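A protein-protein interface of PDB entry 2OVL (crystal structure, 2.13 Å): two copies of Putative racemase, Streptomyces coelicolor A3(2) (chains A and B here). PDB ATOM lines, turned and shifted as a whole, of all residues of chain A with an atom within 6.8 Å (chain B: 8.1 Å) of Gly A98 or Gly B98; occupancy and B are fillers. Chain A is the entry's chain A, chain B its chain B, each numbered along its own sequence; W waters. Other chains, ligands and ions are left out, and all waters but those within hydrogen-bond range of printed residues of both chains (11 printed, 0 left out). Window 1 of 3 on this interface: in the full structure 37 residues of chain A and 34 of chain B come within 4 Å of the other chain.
CB of Ala A94 touches OG of Ser B102, 3.7 Å away. His B252 touches Ala A94. Gly B98 touches Gly A95. His B99 touches Gly A95. Leu B251 touches Arg A96. Gly A97 touches Gly B98 (O to CA, 3.5 Å). CA of Gly A98 touches O of Gly B97 (3.5 Å). Gly A98 touches Gly B98 (CA to CA, 3.8 Å). CE1 of His A99 touches CA of Gly B95 (3.4 Å). CE1 of His A252 touches C of Ala B94 (3.6 Å).
Hydrophobic or aromatic side chains of chain A within 4 Å of the printed part of chain B: Ala A94, His A99 and His A252. Printed residues of chain B that touch a printed residue of chain A: Leu B91, Tyr B93, Ala B94, Gly B95, Gly B97, Gly B98, His B99, Ser B102, Asn B250, Leu B251, His B252 and Asp B256. Hydrophobic or aromatic side chains of chain B that line the printed part of chain A: Ala B94, His B99, Leu B251 and His B252. Among the printed residues, 22 pairs touch across the chains. Among the printed residues, Asp or Glu carboxylates within 4 Å of a Lys or Arg side-chain nitrogen of the other chain: Arg A96 with Asp B256 (3.2 Å).
Gly A98 touches four residues of chain B. Of chain B, only Gly B98 (3.5 Å) comes within 4 Å of Gly A97. Printed residues of chain B within 4 Å of His A252: Ala B94 (3.6 Å) and Gly B95 (3.3 Å). Of the printed residues of chain B, Ser A102 touches Ala B94. Met A63 touches none of the printed residues of chain B.
Water W8 lies within hydrogen-bond range of ND1 of His B99 (2.6 Å), O of Gly A97 (2.9 Å), N of Ala A100 (3.0 Å) and N of His A99 (3.4 Å). Water W9 lies within hydrogen-bond range of O of Arg A96 (2.8 Å), O of Gly A95 (2.9 Å), N of Gly B98 (3.0 Å) and ND1 of His B252 (3.2 Å). Water W6 lies within hydrogen-bond range of the backbone NH (N) of Gly A98, the backbone carbonyl oxygen (O) of Gly B95, a ring nitrogen (ND1) of His A252 and the backbone carbonyl oxygen (O) of Arg B96.
N of His B252 sits at hydrogen-bond distance from OD2 of Asp B256. The backbone carbonyl oxygen (O) of Asn B250 sits close to a ring nitrogen (NE2) of His B252 (3.4 Å). O of Gly A98 is in hydrogen-bond range of OG1 of Thr A101 (3.1 Å). The backbone carbonyl oxygen (O) of Leu B251 sits close to the side-chain amide oxygen (OD1) of Asn B275, at 3.3 Å. The side-chain hydroxyl (OG1) of Thr B253 lies within hydrogen-bond range of the backbone NH (N) of Asp B256.
Ala A94 touches Gly B98, and with the chains exchanged Gly A98 touches Ala B94. Gly A95 touches Gly B98, and with the chains exchanged Gly A98 touches Gly B95. Gly A97 touches Gly B98, and with the chains exchanged Gly A98 touches Gly B97. Gly A98 touches its own counterpart, Gly B98. 14 positions are printed for both chains. Of the 22 pairs that touch across the chains among the printed residues, 17 have their exchanged pair printed and touching as well.
ND1 of His B252 lies within hydrogen-bond range of O of Gly A95 (3.4 Å). O of Asn B250 sits at hydrogen-bond distance from NH2 of Arg A96 (2.7 Å). The backbone carbonyl oxygen (O) of Gly B98 sits close to the backbone carbonyl oxygen (O) of Ala A94, at 3.3 Å. O of Gly A98 lies close to O of Ala B94 (3.2 Å). The backbone NH of His B99 sits at hydrogen-bond distance from the backbone carbonyl oxygen of Ala A94. The backbone carbonyl oxygen of Tyr B93 sits at hydrogen-bond distance from a ring nitrogen (NE2) of His A99, 3.4 Å away. O of Gly B95 lies within hydrogen-bond range of ND1 of His A252 (3.3 Å). The backbone NH (N) of His A99 lies within hydrogen-bond range of the backbone carbonyl oxygen (O) of Ala B94 (2.8 Å). OD2 of Asp B256 is in salt-bridge range of NH2 of Arg A96 (3.2 Å).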
ATOM      1  N   MET A  63       3.991 -24.118  -7.784  1.00  0.00           N
ATOM      2  CA  MET A  63       3.265 -24.699  -8.902  1.00  0.00           C
ATOM      3  C   MET A  63       3.053 -26.184  -8.650  1.00  0.00           C
ATOM      4  O   MET A  63       1.965 -26.709  -8.879  1.00  0.00           O
ATOM      5  CB  MET A  63       4.031 -24.486 -10.203  1.00  0.00           C
ATOM      6  CG  MET A  63       4.186 -23.029 -10.554  1.00  0.00           C
ATOM      7  SD  MET A  63       5.214 -22.787 -12.154  1.00  0.00           S
ATOM      8  CE  MET A  63       6.824 -23.687 -11.652  1.00  0.00           C
ATOM      9  N   ALA A  94      -1.186 -18.729 -19.423  1.00  0.00           N
ATOM     10  CA  ALA A  94      -0.065 -17.916 -18.945  1.00  0.00           C
ATOM     11  C   ALA A  94       1.225 -18.725 -18.834  1.00  0.00           C
ATOM     12  O   ALA A  94       2.275 -18.185 -18.472  1.00  0.00           O
ATOM     13  CB  ALA A  94      -0.399 -17.271 -17.568  1.00  0.00           C
ATOM     14  N   GLY A  95       1.146 -20.019 -19.138  1.00  0.00           N
ATOM     15  CA  GLY A  95       2.325 -20.869 -19.069  1.00  0.00           C
ATOM     16  C   GLY A  95       2.889 -21.213 -20.438  1.00  0.00           C
ATOM     17  O   GLY A  95       3.473 -20.352 -21.107  1.00  0.00           O
ATOM     18  N   ARG A  96       2.727 -22.472 -20.855  1.00  0.00           N
ATOM     19  CA  ARG A  96       3.217 -22.931 -22.162  1.00  0.00           C
ATOM     20  C   ARG A  96       4.663 -22.479 -22.331  1.00  0.00           C
ATOM     21  O   ARG A  96       5.006 -21.751 -23.267  1.00  0.00           O
ATOM     22  CB  ARG A  96       2.343 -22.341 -23.273  1.00  0.00           C
ATOM     23  CG  ARG A  96       2.604 -22.885 -24.668  1.00  0.00           C
ATOM     24  CD  ARG A  96       1.771 -22.113 -25.677  1.00  0.00           C
ATOM     25  NE  ARG A  96       2.182 -20.713 -25.725  1.00  0.00           N
ATOM     26  CZ  ARG A  96       3.326 -20.293 -26.253  1.00  0.00           C
ATOM     27  NH1 ARG A  96       4.167 -21.168 -26.791  1.00  0.00           N
ATOM     28  NH2 ARG A  96       3.652 -19.002 -26.209  1.00  0.00           N
ATOM     29  N   GLY A  97       5.500 -22.931 -21.403  1.00  0.00           N
ATOM     30  CA  GLY A  97       6.902 -22.562 -21.380  1.00  0.00           C
ATOM     31  C   GLY A  97       7.118 -21.958 -20.002  1.00  0.00           C
ATOM     32  O   GLY A  97       6.201 -21.985 -19.176  1.00  0.00           O
ATOM     33  N   GLY A  98       8.307 -21.429 -19.731  1.00  0.00           N
ATOM     34  CA  GLY A  98       8.550 -20.828 -18.429  1.00  0.00           C
ATOM     35  C   GLY A  98       8.718 -21.794 -17.262  1.00  0.00           C
ATOM     36  O   GLY A  98       8.904 -22.996 -17.452  1.00  0.00           O
ATOM     37  N   HIS A  99       8.642 -21.256 -16.046  1.00  0.00           N
ATOM     38  CA  HIS A  99       8.812 -22.040 -14.826  1.00  0.00           C
ATOM     39  C   HIS A  99       7.907 -23.258 -14.699  1.00  0.00           C
ATOM     40  O   HIS A  99       8.272 -24.221 -14.036  1.00  0.00           O
ATOM     41  CB  HIS A  99       8.661 -21.133 -13.588  1.00  0.00           C
ATOM     42  CG  HIS A  99       9.758 -20.120 -13.453  1.00  0.00           C
ATOM     43  ND1 HIS A  99       9.857 -19.016 -14.275  1.00  0.00           N
ATOM     44  CD2 HIS A  99      10.843 -20.084 -12.643  1.00  0.00           C
ATOM     45  CE1 HIS A  99      10.955 -18.345 -13.979  1.00  0.00           C
ATOM     46  NE2 HIS A  99      11.574 -18.971 -12.994  1.00  0.00           N
ATOM     47  N   ALA A 100       6.735 -23.219 -15.326  1.00  0.00           N
ATOM     48  CA  ALA A 100       5.816 -24.347 -15.277  1.00  0.00           C
ATOM     49  C   ALA A 100       6.451 -25.629 -15.811  1.00  0.00           C
ATOM     50  O   ALA A 100       6.133 -26.724 -15.335  1.00  0.00           O
ATOM     51  CB  ALA A 100       4.553 -24.037 -16.065  1.00  0.00           C
ATOM     52  N   THR A 101       7.351 -25.503 -16.789  1.00  0.00           N
ATOM     53  CA  THR A 101       7.992 -26.686 -17.367  1.00  0.00           C
ATOM     54  C   THR A 101       8.992 -27.333 -16.408  1.00  0.00           C
ATOM     55  O   THR A 101       9.240 -28.535 -16.491  1.00  0.00           O
ATOM     56  CB  THR A 101       8.693 -26.371 -18.735  1.00  0.00           C
ATOM     57  OG1 THR A 101       9.935 -25.692 -18.522  1.00  0.00           O
ATOM     58  CG2 THR A 101       7.792 -25.503 -19.602  1.00  0.00           C
ATOM     59  N   SER A 102       9.566 -26.543 -15.501  1.00  0.00           N
ATOM     60  CA  SER A 102      10.507 -27.078 -14.514  1.00  0.00           C
ATOM     61  C   SER A 102       9.711 -27.846 -13.462  1.00  0.00           C
ATOM     62  O   SER A 102      10.140 -28.897 -12.988  1.00  0.00           O
ATOM     63  CB  SER A 102      11.297 -25.949 -13.839  1.00  0.00           C
ATOM     64  OG  SER A 102      12.342 -25.488 -14.675  1.00  0.00           O
ATOM     65  N   ALA A 103       8.555 -27.299 -13.094  1.00  0.00           N
ATOM     66  CA  ALA A 103       7.677 -27.935 -12.123  1.00  0.00           C
ATOM     67  C   ALA A 103       7.259 -29.289 -12.686  1.00  0.00           C
ATOM     68  O   ALA A 103       7.259 -30.299 -11.980  1.00  0.00           O
ATOM     69  CB  ALA A 103       6.439 -27.070 -11.892  1.00  0.00           C
ATOM     70  N   HIS A 252      12.514 -24.671 -23.414  1.00  0.00           N
ATOM     71  CA  HIS A 252      11.664 -25.360 -22.445  1.00  0.00           C
ATOM     72  C   HIS A 252      10.517 -26.216 -22.937  1.00  0.00           C
ATOM     73  O   HIS A 252       9.749 -26.749 -22.131  1.00  0.00           O
ATOM     74  CB  HIS A 252      11.135 -24.319 -21.460  1.00  0.00           C
ATOM     75  CG  HIS A 252      12.224 -23.573 -20.752  1.00  0.00           C
ATOM     76  ND1 HIS A 252      12.175 -22.214 -20.527  1.00  0.00           N
ATOM     77  CD2 HIS A 252      13.405 -23.999 -20.239  1.00  0.00           C
ATOM     78  CE1 HIS A 252      13.282 -21.834 -19.912  1.00  0.00           C
ATOM     79  NE2 HIS A 252      14.044 -22.898 -19.726  1.00  0.00           N
ATOM     80  N   THR A 253      10.381 -26.344 -24.248  1.00  0.00           N
ATOM     81  CA  THR A 253       9.323 -27.180 -24.799  1.00  0.00           C
ATOM     82  C   THR A 253       9.885 -27.939 -25.983  1.00  0.00           C
ATOM     83  O   THR A 253      10.918 -27.570 -26.544  1.00  0.00           O
ATOM     84  CB  THR A 253       8.109 -26.353 -25.285  1.00  0.00           C
ATOM     85  OG1 THR A 253       8.474 -25.597 -26.450  1.00  0.00           O
ATOM     86  CG2 THR A 253       7.635 -25.397 -24.189  1.00  0.00           C
ATOM     87  N   ASN A 275      14.197 -29.128 -16.895  1.00  0.00           N
ATOM     88  CA  ASN A 275      13.352 -27.999 -17.297  1.00  0.00           C
ATOM     89  C   ASN A 275      12.677 -28.209 -18.654  1.00  0.00           C
ATOM     90  O   ASN A 275      11.756 -27.471 -19.012  1.00  0.00           O
ATOM     91  CB  ASN A 275      14.131 -26.665 -17.288  1.00  0.00           C
ATOM     92  CG  ASN A 275      15.090 -26.518 -18.461  1.00  0.00           C
ATOM     93  OD1 ASN A 275      14.759 -26.840 -19.604  1.00  0.00           O
ATOM     94  ND2 ASN A 275      16.274 -25.996 -18.185  1.00  0.00           N
ATOM     95  N   VAL B  60       2.339 -16.718  -9.674  1.00  0.00           N
ATOM     96  CA  VAL B  60       2.559 -15.377 -10.213  1.00  0.00           C
ATOM     97  C   VAL B  60       2.816 -14.362  -9.099  1.00  0.00           C
ATOM     98  O   VAL B  60       3.769 -13.580  -9.164  1.00  0.00           O
ATOM     99  CB  VAL B  60       1.349 -14.911 -11.044  1.00  0.00           C
ATOM    100  CG1 VAL B  60       1.550 -13.469 -11.495  1.00  0.00           C
ATOM    101  CG2 VAL B  60       1.182 -15.825 -12.266  1.00  0.00           C
ATOM    102  N   MET B  63       6.176 -14.735  -7.605  1.00  0.00           N
ATOM    103  CA  MET B  63       7.254 -14.181  -8.416  1.00  0.00           C
ATOM    104  C   MET B  63       7.406 -12.679  -8.181  1.00  0.00           C
ATOM    105  O   MET B  63       8.515 -12.174  -8.014  1.00  0.00           O
ATOM    106  CB  MET B  63       6.991 -14.453  -9.898  1.00  0.00           C
ATOM    107  CG  MET B  63       7.111 -15.916 -10.276  1.00  0.00           C
ATOM    108  SD  MET B  63       6.596 -16.256 -12.113  1.00  0.00           S
ATOM    109  CE  MET B  63       4.732 -16.389 -11.900  1.00  0.00           C
ATOM    110  N   TRP B  88      13.124  -9.140 -16.421  1.00  0.00           N
ATOM    111  CA  TRP B  88      13.197 -10.182 -17.444  1.00  0.00           C
ATOM    112  C   TRP B  88      14.392 -11.078 -17.144  1.00  0.00           C
ATOM    113  O   TRP B  88      14.286 -12.306 -17.180  1.00  0.00           O
ATOM    114  CB  TRP B  88      13.334  -9.528 -18.830  1.00  0.00           C
ATOM    115  CG  TRP B  88      13.637 -10.466 -19.977  1.00  0.00           C
ATOM    116  CD1 TRP B  88      14.839 -10.622 -20.616  1.00  0.00           C
ATOM    117  CD2 TRP B  88      12.717 -11.355 -20.630  1.00  0.00           C
ATOM    118  NE1 TRP B  88      14.720 -11.551 -21.632  1.00  0.00           N
ATOM    119  CE2 TRP B  88      13.429 -12.015 -21.659  1.00  0.00           C
ATOM    120  CE3 TRP B  88      11.358 -11.653 -20.448  1.00  0.00           C
ATOM    121  CZ2 TRP B  88      12.827 -12.960 -22.502  1.00  0.00           C
ATOM    122  CZ3 TRP B  88      10.756 -12.596 -21.292  1.00  0.00           C
ATOM    123  CH2 TRP B  88      11.495 -13.235 -22.304  1.00  0.00           C
ATOM    124  N   LEU B  91      14.232 -13.350 -13.702  1.00  0.00           N
ATOM    125  CA  LEU B  91      13.457 -14.588 -13.818  1.00  0.00           C
ATOM    126  C   LEU B  91      13.748 -15.345 -15.119  1.00  0.00           C
ATOM    127  O   LEU B  91      12.975 -16.213 -15.527  1.00  0.00           O
ATOM    128  CB  LEU B  91      11.956 -14.274 -13.750  1.00  0.00           C
ATOM    129  CG  LEU B  91      11.384 -13.813 -12.403  1.00  0.00           C
ATOM    130  CD1 LEU B  91       9.931 -13.407 -12.560  1.00  0.00           C
ATOM    131  CD2 LEU B  91      11.506 -14.949 -11.400  1.00  0.00           C
ATOM    132  N   HIS B  92      14.866 -15.032 -15.761  1.00  0.00           N
ATOM    133  CA  HIS B  92      15.213 -15.675 -17.027  1.00  0.00           C
ATOM    134  C   HIS B  92      15.553 -17.167 -16.930  1.00  0.00           C
ATOM    135  O   HIS B  92      15.164 -17.946 -17.799  1.00  0.00           O
ATOM    136  CB  HIS B  92      16.365 -14.917 -17.694  1.00  0.00           C
ATOM    137  CG  HIS B  92      16.521 -15.213 -19.156  1.00  0.00           C
ATOM    138  ND1 HIS B  92      17.167 -16.335 -19.627  1.00  0.00           N
ATOM    139  CD2 HIS B  92      16.107 -14.531 -20.251  1.00  0.00           C
ATOM    140  CE1 HIS B  92      17.148 -16.332 -20.948  1.00  0.00           C
ATOM    141  NE2 HIS B  92      16.510 -15.248 -21.352  1.00  0.00           N
ATOM    142  N   TYR B  93      16.282 -17.580 -15.902  1.00  0.00           N
ATOM    143  CA  TYR B  93      16.601 -19.003 -15.801  1.00  0.00           C
ATOM    144  C   TYR B  93      15.307 -19.750 -15.467  1.00  0.00           C
ATOM    145  O   TYR B  93      14.647 -19.442 -14.473  1.00  0.00           O
ATOM    146  CB  TYR B  93      17.663 -19.280 -14.727  1.00  0.00           C
ATOM    147  CG  TYR B  93      18.144 -20.712 -14.795  1.00  0.00           C
ATOM    148  CD1 TYR B  93      18.985 -21.131 -15.826  1.00  0.00           C
ATOM    149  CD2 TYR B  93      17.670 -21.673 -13.901  1.00  0.00           C
ATOM    150  CE1 TYR B  93      19.340 -22.476 -15.976  1.00  0.00           C
ATOM    151  CE2 TYR B  93      18.014 -23.020 -14.037  1.00  0.00           C
ATOM    152  CZ  TYR B  93      18.847 -23.418 -15.080  1.00  0.00           C
ATOM    153  OH  TYR B  93      19.168 -24.754 -15.249  1.00  0.00           O
ATOM    154  N   ALA B  94      14.954 -20.722 -16.310  1.00  0.00           N
ATOM    155  CA  ALA B  94      13.729 -21.521 -16.164  1.00  0.00           C
ATOM    156  C   ALA B  94      12.496 -20.707 -16.553  1.00  0.00           C
ATOM    157  O   ALA B  94      11.369 -21.211 -16.514  1.00  0.00           O
ATOM    158  CB  ALA B  94      13.579 -22.046 -14.729  1.00  0.00           C
ATOM    159  N   GLY B  95      12.718 -19.448 -16.925  1.00  0.00           N
ATOM    160  CA  GLY B  95      11.626 -18.578 -17.321  1.00  0.00           C
ATOM    161  C   GLY B  95      11.676 -18.275 -18.814  1.00  0.00           C
ATOM    162  O   GLY B  95      11.417 -19.163 -19.632  1.00  0.00           O
ATOM    163  N   ARG B  96      12.021 -17.036 -19.176  1.00  0.00           N
ATOM    164  CA  ARG B  96      12.082 -16.629 -20.590  1.00  0.00           C
ATOM    165  C   ARG B  96      10.770 -17.043 -21.269  1.00  0.00           C
ATOM    166  O   ARG B  96      10.756 -17.719 -22.301  1.00  0.00           O
ATOM    167  CB  ARG B  96      13.276 -17.296 -21.287  1.00  0.00           C
ATOM    168  CG  ARG B  96      13.582 -16.772 -22.689  1.00  0.00           C
ATOM    169  CD  ARG B  96      14.660 -17.633 -23.350  1.00  0.00           C
ATOM    170  NE  ARG B  96      14.217 -19.022 -23.468  1.00  0.00           N
ATOM    171  CZ  ARG B  96      13.316 -19.445 -24.349  1.00  0.00           C
ATOM    172  NH1 ARG B  96      12.768 -18.588 -25.198  1.00  0.00           N
ATOM    173  NH2 ARG B  96      12.930 -20.718 -24.356  1.00  0.00           N
ATOM    174  N   GLY B  97       9.672 -16.606 -20.666  1.00  0.00           N
ATOM    175  CA  GLY B  97       8.347 -16.921 -21.152  1.00  0.00           C
ATOM    176  C   GLY B  97       7.600 -17.459 -19.947  1.00  0.00           C
ATOM    177  O   GLY B  97       8.122 -17.401 -18.834  1.00  0.00           O
ATOM    178  N   GLY B  98       6.395 -17.978 -20.150  1.00  0.00           N
ATOM    179  CA  GLY B  98       5.643 -18.515 -19.035  1.00  0.00           C
ATOM    180  C   GLY B  98       5.084 -17.476 -18.076  1.00  0.00           C
ATOM    181  O   GLY B  98       5.010 -16.282 -18.393  1.00  0.00           O
ATOM    182  N   HIS B  99       4.699 -17.950 -16.893  1.00  0.00           N
ATOM    183  CA  HIS B  99       4.099 -17.127 -15.849  1.00  0.00           C
ATOM    184  C   HIS B  99       4.908 -15.901 -15.455  1.00  0.00           C
ATOM    185  O   HIS B  99       4.340 -14.883 -15.080  1.00  0.00           O
ATOM    186  CB  HIS B  99       3.806 -17.993 -14.615  1.00  0.00           C
ATOM    187  CG  HIS B  99       2.763 -19.035 -14.860  1.00  0.00           C
ATOM    188  ND1 HIS B  99       2.997 -20.153 -15.629  1.00  0.00           N
ATOM    189  CD2 HIS B  99       1.458 -19.090 -14.503  1.00  0.00           C
ATOM    190  CE1 HIS B  99       1.881 -20.851 -15.741  1.00  0.00           C
ATOM    191  NE2 HIS B  99       0.931 -20.227 -15.070  1.00  0.00           N
ATOM    192  N   ALA B 100       6.226 -15.998 -15.523  1.00  0.00           N
ATOM    193  CA  ALA B 100       7.059 -14.850 -15.202  1.00  0.00           C
ATOM    194  C   ALA B 100       6.646 -13.632 -16.039  1.00  0.00           C
ATOM    195  O   ALA B 100       6.779 -12.500 -15.574  1.00  0.00           O
ATOM    196  CB  ALA B 100       8.520 -15.168 -15.459  1.00  0.00           C
ATOM    197  N   THR B 101       6.143 -13.849 -17.258  1.00  0.00           N
ATOM    198  CA  THR B 101       5.773 -12.700 -18.097  1.00  0.00           C
ATOM    199  C   THR B 101       4.502 -12.001 -17.618  1.00  0.00           C
ATOM    200  O   THR B 101       4.297 -10.810 -17.890  1.00  0.00           O
ATOM    201  CB  THR B 101       5.647 -13.081 -19.610  1.00  0.00           C
ATOM    202  OG1 THR B 101       4.409 -13.762 -19.869  1.00  0.00           O
ATOM    203  CG2 THR B 101       6.819 -13.982 -20.021  1.00  0.00           C
ATOM    204  N   SER B 102       3.652 -12.734 -16.901  1.00  0.00           N
ATOM    205  CA  SER B 102       2.421 -12.157 -16.358  1.00  0.00           C
ATOM    206  C   SER B 102       2.789 -11.362 -15.101  1.00  0.00           C
ATOM    207  O   SER B 102       2.220 -10.304 -14.829  1.00  0.00           O
ATOM    208  CB  SER B 102       1.415 -13.255 -16.007  1.00  0.00           C
ATOM    209  OG  SER B 102       0.820 -13.796 -17.176  1.00  0.00           O
ATOM    210  N   ALA B 103       3.743 -11.886 -14.338  1.00  0.00           N
ATOM    211  CA  ALA B 103       4.219 -11.213 -13.138  1.00  0.00           C
ATOM    212  C   ALA B 103       4.822  -9.888 -13.590  1.00  0.00           C
ATOM    213  O   ALA B 103       4.546  -8.835 -13.016  1.00  0.00           O
ATOM    214  CB  ALA B 103       5.284 -12.054 -12.448  1.00  0.00           C
ATOM    215  N   ILE B 104       5.655  -9.963 -14.627  1.00  0.00           N
ATOM    216  CA  ILE B 104       6.304  -8.787 -15.186  1.00  0.00           C
ATOM    217  C   ILE B 104       5.294  -7.751 -15.686  1.00  0.00           C
ATOM    218  O   ILE B 104       5.454  -6.557 -15.423  1.00  0.00           O
ATOM    219  CB  ILE B 104       7.271  -9.191 -16.327  1.00  0.00           C
ATOM    220  CG1 ILE B 104       8.510  -9.858 -15.714  1.00  0.00           C
ATOM    221  CG2 ILE B 104       7.648  -7.971 -17.162  1.00  0.00           C
ATOM    222  CD1 ILE B 104       9.539 -10.366 -16.702  1.00  0.00           C
ATOM    223  N   SER B 105       4.255  -8.213 -16.380  1.00  0.00           N
ATOM    224  CA  SER B 105       3.214  -7.330 -16.915  1.00  0.00           C
ATOM    225  C   SER B 105       2.505  -6.535 -15.813  1.00  0.00           C
ATOM    226  O   SER B 105       2.238  -5.343 -15.973  1.00  0.00           O
ATOM    227  CB  SER B 105       2.155  -8.133 -17.682  1.00  0.00           C
ATOM    228  OG  SER B 105       2.730  -8.930 -18.700  1.00  0.00           O
ATOM    229  N   ASN B 250      -1.923 -16.339 -26.224  1.00  0.00           N
ATOM    230  CA  ASN B 250      -1.053 -17.311 -25.574  1.00  0.00           C
ATOM    231  C   ASN B 250       0.426 -17.129 -25.902  1.00  0.00           C
ATOM    232  O   ASN B 250       1.265 -17.937 -25.496  1.00  0.00           O
ATOM    233  CB  ASN B 250      -1.523 -18.732 -25.895  1.00  0.00           C
ATOM    234  CG  ASN B 250      -2.707 -19.152 -25.032  1.00  0.00           C
ATOM    235  OD1 ASN B 250      -2.571 -19.328 -23.818  1.00  0.00           O
ATOM    236  ND2 ASN B 250      -3.872 -19.292 -25.647  1.00  0.00           N
ATOM    237  N   LEU B 251       0.743 -16.067 -26.641  1.00  0.00           N
ATOM    238  CA  LEU B 251       2.132 -15.753 -26.960  1.00  0.00           C
ATOM    239  C   LEU B 251       2.563 -14.840 -25.800  1.00  0.00           C
ATOM    240  O   LEU B 251       1.834 -13.931 -25.410  1.00  0.00           O
ATOM    241  CB  LEU B 251       2.230 -15.040 -28.314  1.00  0.00           C
ATOM    242  CG  LEU B 251       1.717 -15.889 -29.492  1.00  0.00           C
ATOM    243  CD1 LEU B 251       1.935 -15.156 -30.819  1.00  0.00           C
ATOM    244  CD2 LEU B 251       2.457 -17.226 -29.518  1.00  0.00           C
ATOM    245  N   HIS B 252       3.742 -15.075 -25.245  1.00  0.00           N
ATOM    246  CA  HIS B 252       4.161 -14.305 -24.079  1.00  0.00           C
ATOM    247  C   HIS B 252       5.434 -13.486 -24.174  1.00  0.00           C
ATOM    248  O   HIS B 252       5.894 -12.935 -23.167  1.00  0.00           O
ATOM    249  CB  HIS B 252       4.232 -15.261 -22.887  1.00  0.00           C
ATOM    250  CG  HIS B 252       2.932 -15.960 -22.622  1.00  0.00           C
ATOM    251  ND1 HIS B 252       2.845 -17.314 -22.378  1.00  0.00           N
ATOM    252  CD2 HIS B 252       1.659 -15.495 -22.619  1.00  0.00           C
ATOM    253  CE1 HIS B 252       1.574 -17.653 -22.241  1.00  0.00           C
ATOM    254  NE2 HIS B 252       0.834 -16.567 -22.384  1.00  0.00           N
ATOM    255  N   THR B 253       6.011 -13.408 -25.368  1.00  0.00           N
ATOM    256  CA  THR B 253       7.215 -12.612 -25.550  1.00  0.00           C
ATOM    257  C   THR B 253       7.166 -11.926 -26.901  1.00  0.00           C
ATOM    258  O   THR B 253       6.440 -12.346 -27.806  1.00  0.00           O
ATOM    259  CB  THR B 253       8.495 -13.464 -25.497  1.00  0.00           C
ATOM    260  OG1 THR B 253       8.577 -14.268 -26.676  1.00  0.00           O
ATOM    261  CG2 THR B 253       8.498 -14.368 -24.266  1.00  0.00           C
ATOM    262  N   ASP B 256       7.953 -14.288 -29.600  1.00  0.00           N
ATOM    263  CA  ASP B 256       6.881 -15.180 -30.055  1.00  0.00           C
ATOM    264  C   ASP B 256       6.126 -14.488 -31.188  1.00  0.00           C
ATOM    265  O   ASP B 256       5.836 -15.099 -32.216  1.00  0.00           O
ATOM    266  CB  ASP B 256       5.863 -15.465 -28.943  1.00  0.00           C
ATOM    267  CG  ASP B 256       6.297 -16.571 -27.987  1.00  0.00           C
ATOM    268  OD1 ASP B 256       7.198 -17.370 -28.323  1.00  0.00           O
ATOM    269  OD2 ASP B 256       5.697 -16.644 -26.894  1.00  0.00           O
ATOM    270  N   SER B 274      -1.783  -8.050 -20.143  1.00  0.00           N
ATOM    271  CA  SER B 274      -1.538  -8.658 -18.835  1.00  0.00           C
ATOM    272  C   SER B 274      -0.595  -9.866 -18.841  1.00  0.00           C
ATOM    273  O   SER B 274      -0.250 -10.382 -17.780  1.00  0.00           O
ATOM    274  CB  SER B 274      -2.866  -9.042 -18.163  1.00  0.00           C
ATOM    275  OG  SER B 274      -3.487 -10.139 -18.815  1.00  0.00           O
ATOM    276  N   ASN B 275      -0.172 -10.329 -20.015  1.00  0.00           N
ATOM    277  CA  ASN B 275       0.762 -11.458 -20.035  1.00  0.00           C
ATOM    278  C   ASN B 275       1.895 -11.265 -21.040  1.00  0.00           C
ATOM    279  O   ASN B 275       2.903 -11.967 -20.993  1.00  0.00           O
ATOM    280  CB  ASN B 275       0.028 -12.792 -20.302  1.00  0.00           C
ATOM    281  CG  ASN B 275      -0.368 -12.981 -21.767  1.00  0.00           C
ATOM    282  OD1 ASN B 275       0.410 -12.697 -22.677  1.00  0.00           O
ATOM    283  ND2 ASN B 275      -1.575 -13.491 -21.993  1.00  0.00           N
ATOM    284  N   ILE B 276       1.755 -10.291 -21.933  1.00  0.00           N
ATOM    285  CA  ILE B 276       2.793 -10.086 -22.932  1.00  0.00           C
ATOM    286  C   ILE B 276       3.979  -9.263 -22.435  1.00  0.00           C
ATOM    287  O   ILE B 276       4.992  -9.170 -23.116  1.00  0.00           O
ATOM    288  CB  ILE B 276       2.219  -9.422 -24.193  1.00  0.00           C
ATOM    289  CG1 ILE B 276       3.214  -9.573 -25.341  1.00  0.00           C
ATOM    290  CG2 ILE B 276       1.911  -7.951 -23.918  1.00  0.00           C
ATOM    291  CD1 ILE B 276       2.709  -9.013 -26.625  1.00  0.00           C
HETATM  292  O   HOH W   1      17.122 -26.575 -15.414  1.00  0.00           O
HETATM  293  O   HOH W   2      -1.922 -17.305 -21.739  1.00  0.00           O
HETATM  294  O   HOH W   3      16.702 -22.111 -18.053  1.00  0.00           O
HETATM  295  O   HOH W   4       6.690 -19.941 -27.562  1.00  0.00           O
HETATM  296  O   HOH W   5       2.307 -15.344 -18.683  1.00  0.00           O
HETATM  297  O   HOH W   6      10.058 -20.596 -21.764  1.00  0.00           O
HETATM  298  O   HOH W   7      14.075 -17.694 -12.475  1.00  0.00           O
HETATM  299  O   HOH W   8       5.312 -20.924 -16.584  1.00  0.00           O
HETATM  300  O   HOH W   9       5.441 -19.068 -22.758  1.00  0.00           O
HETATM  301  O   HOH W  10       7.834 -18.364 -16.213  1.00  0.00           O
HETATM  302  O   HOH W  11      11.436 -24.056 -16.789  1.00  0.00           O
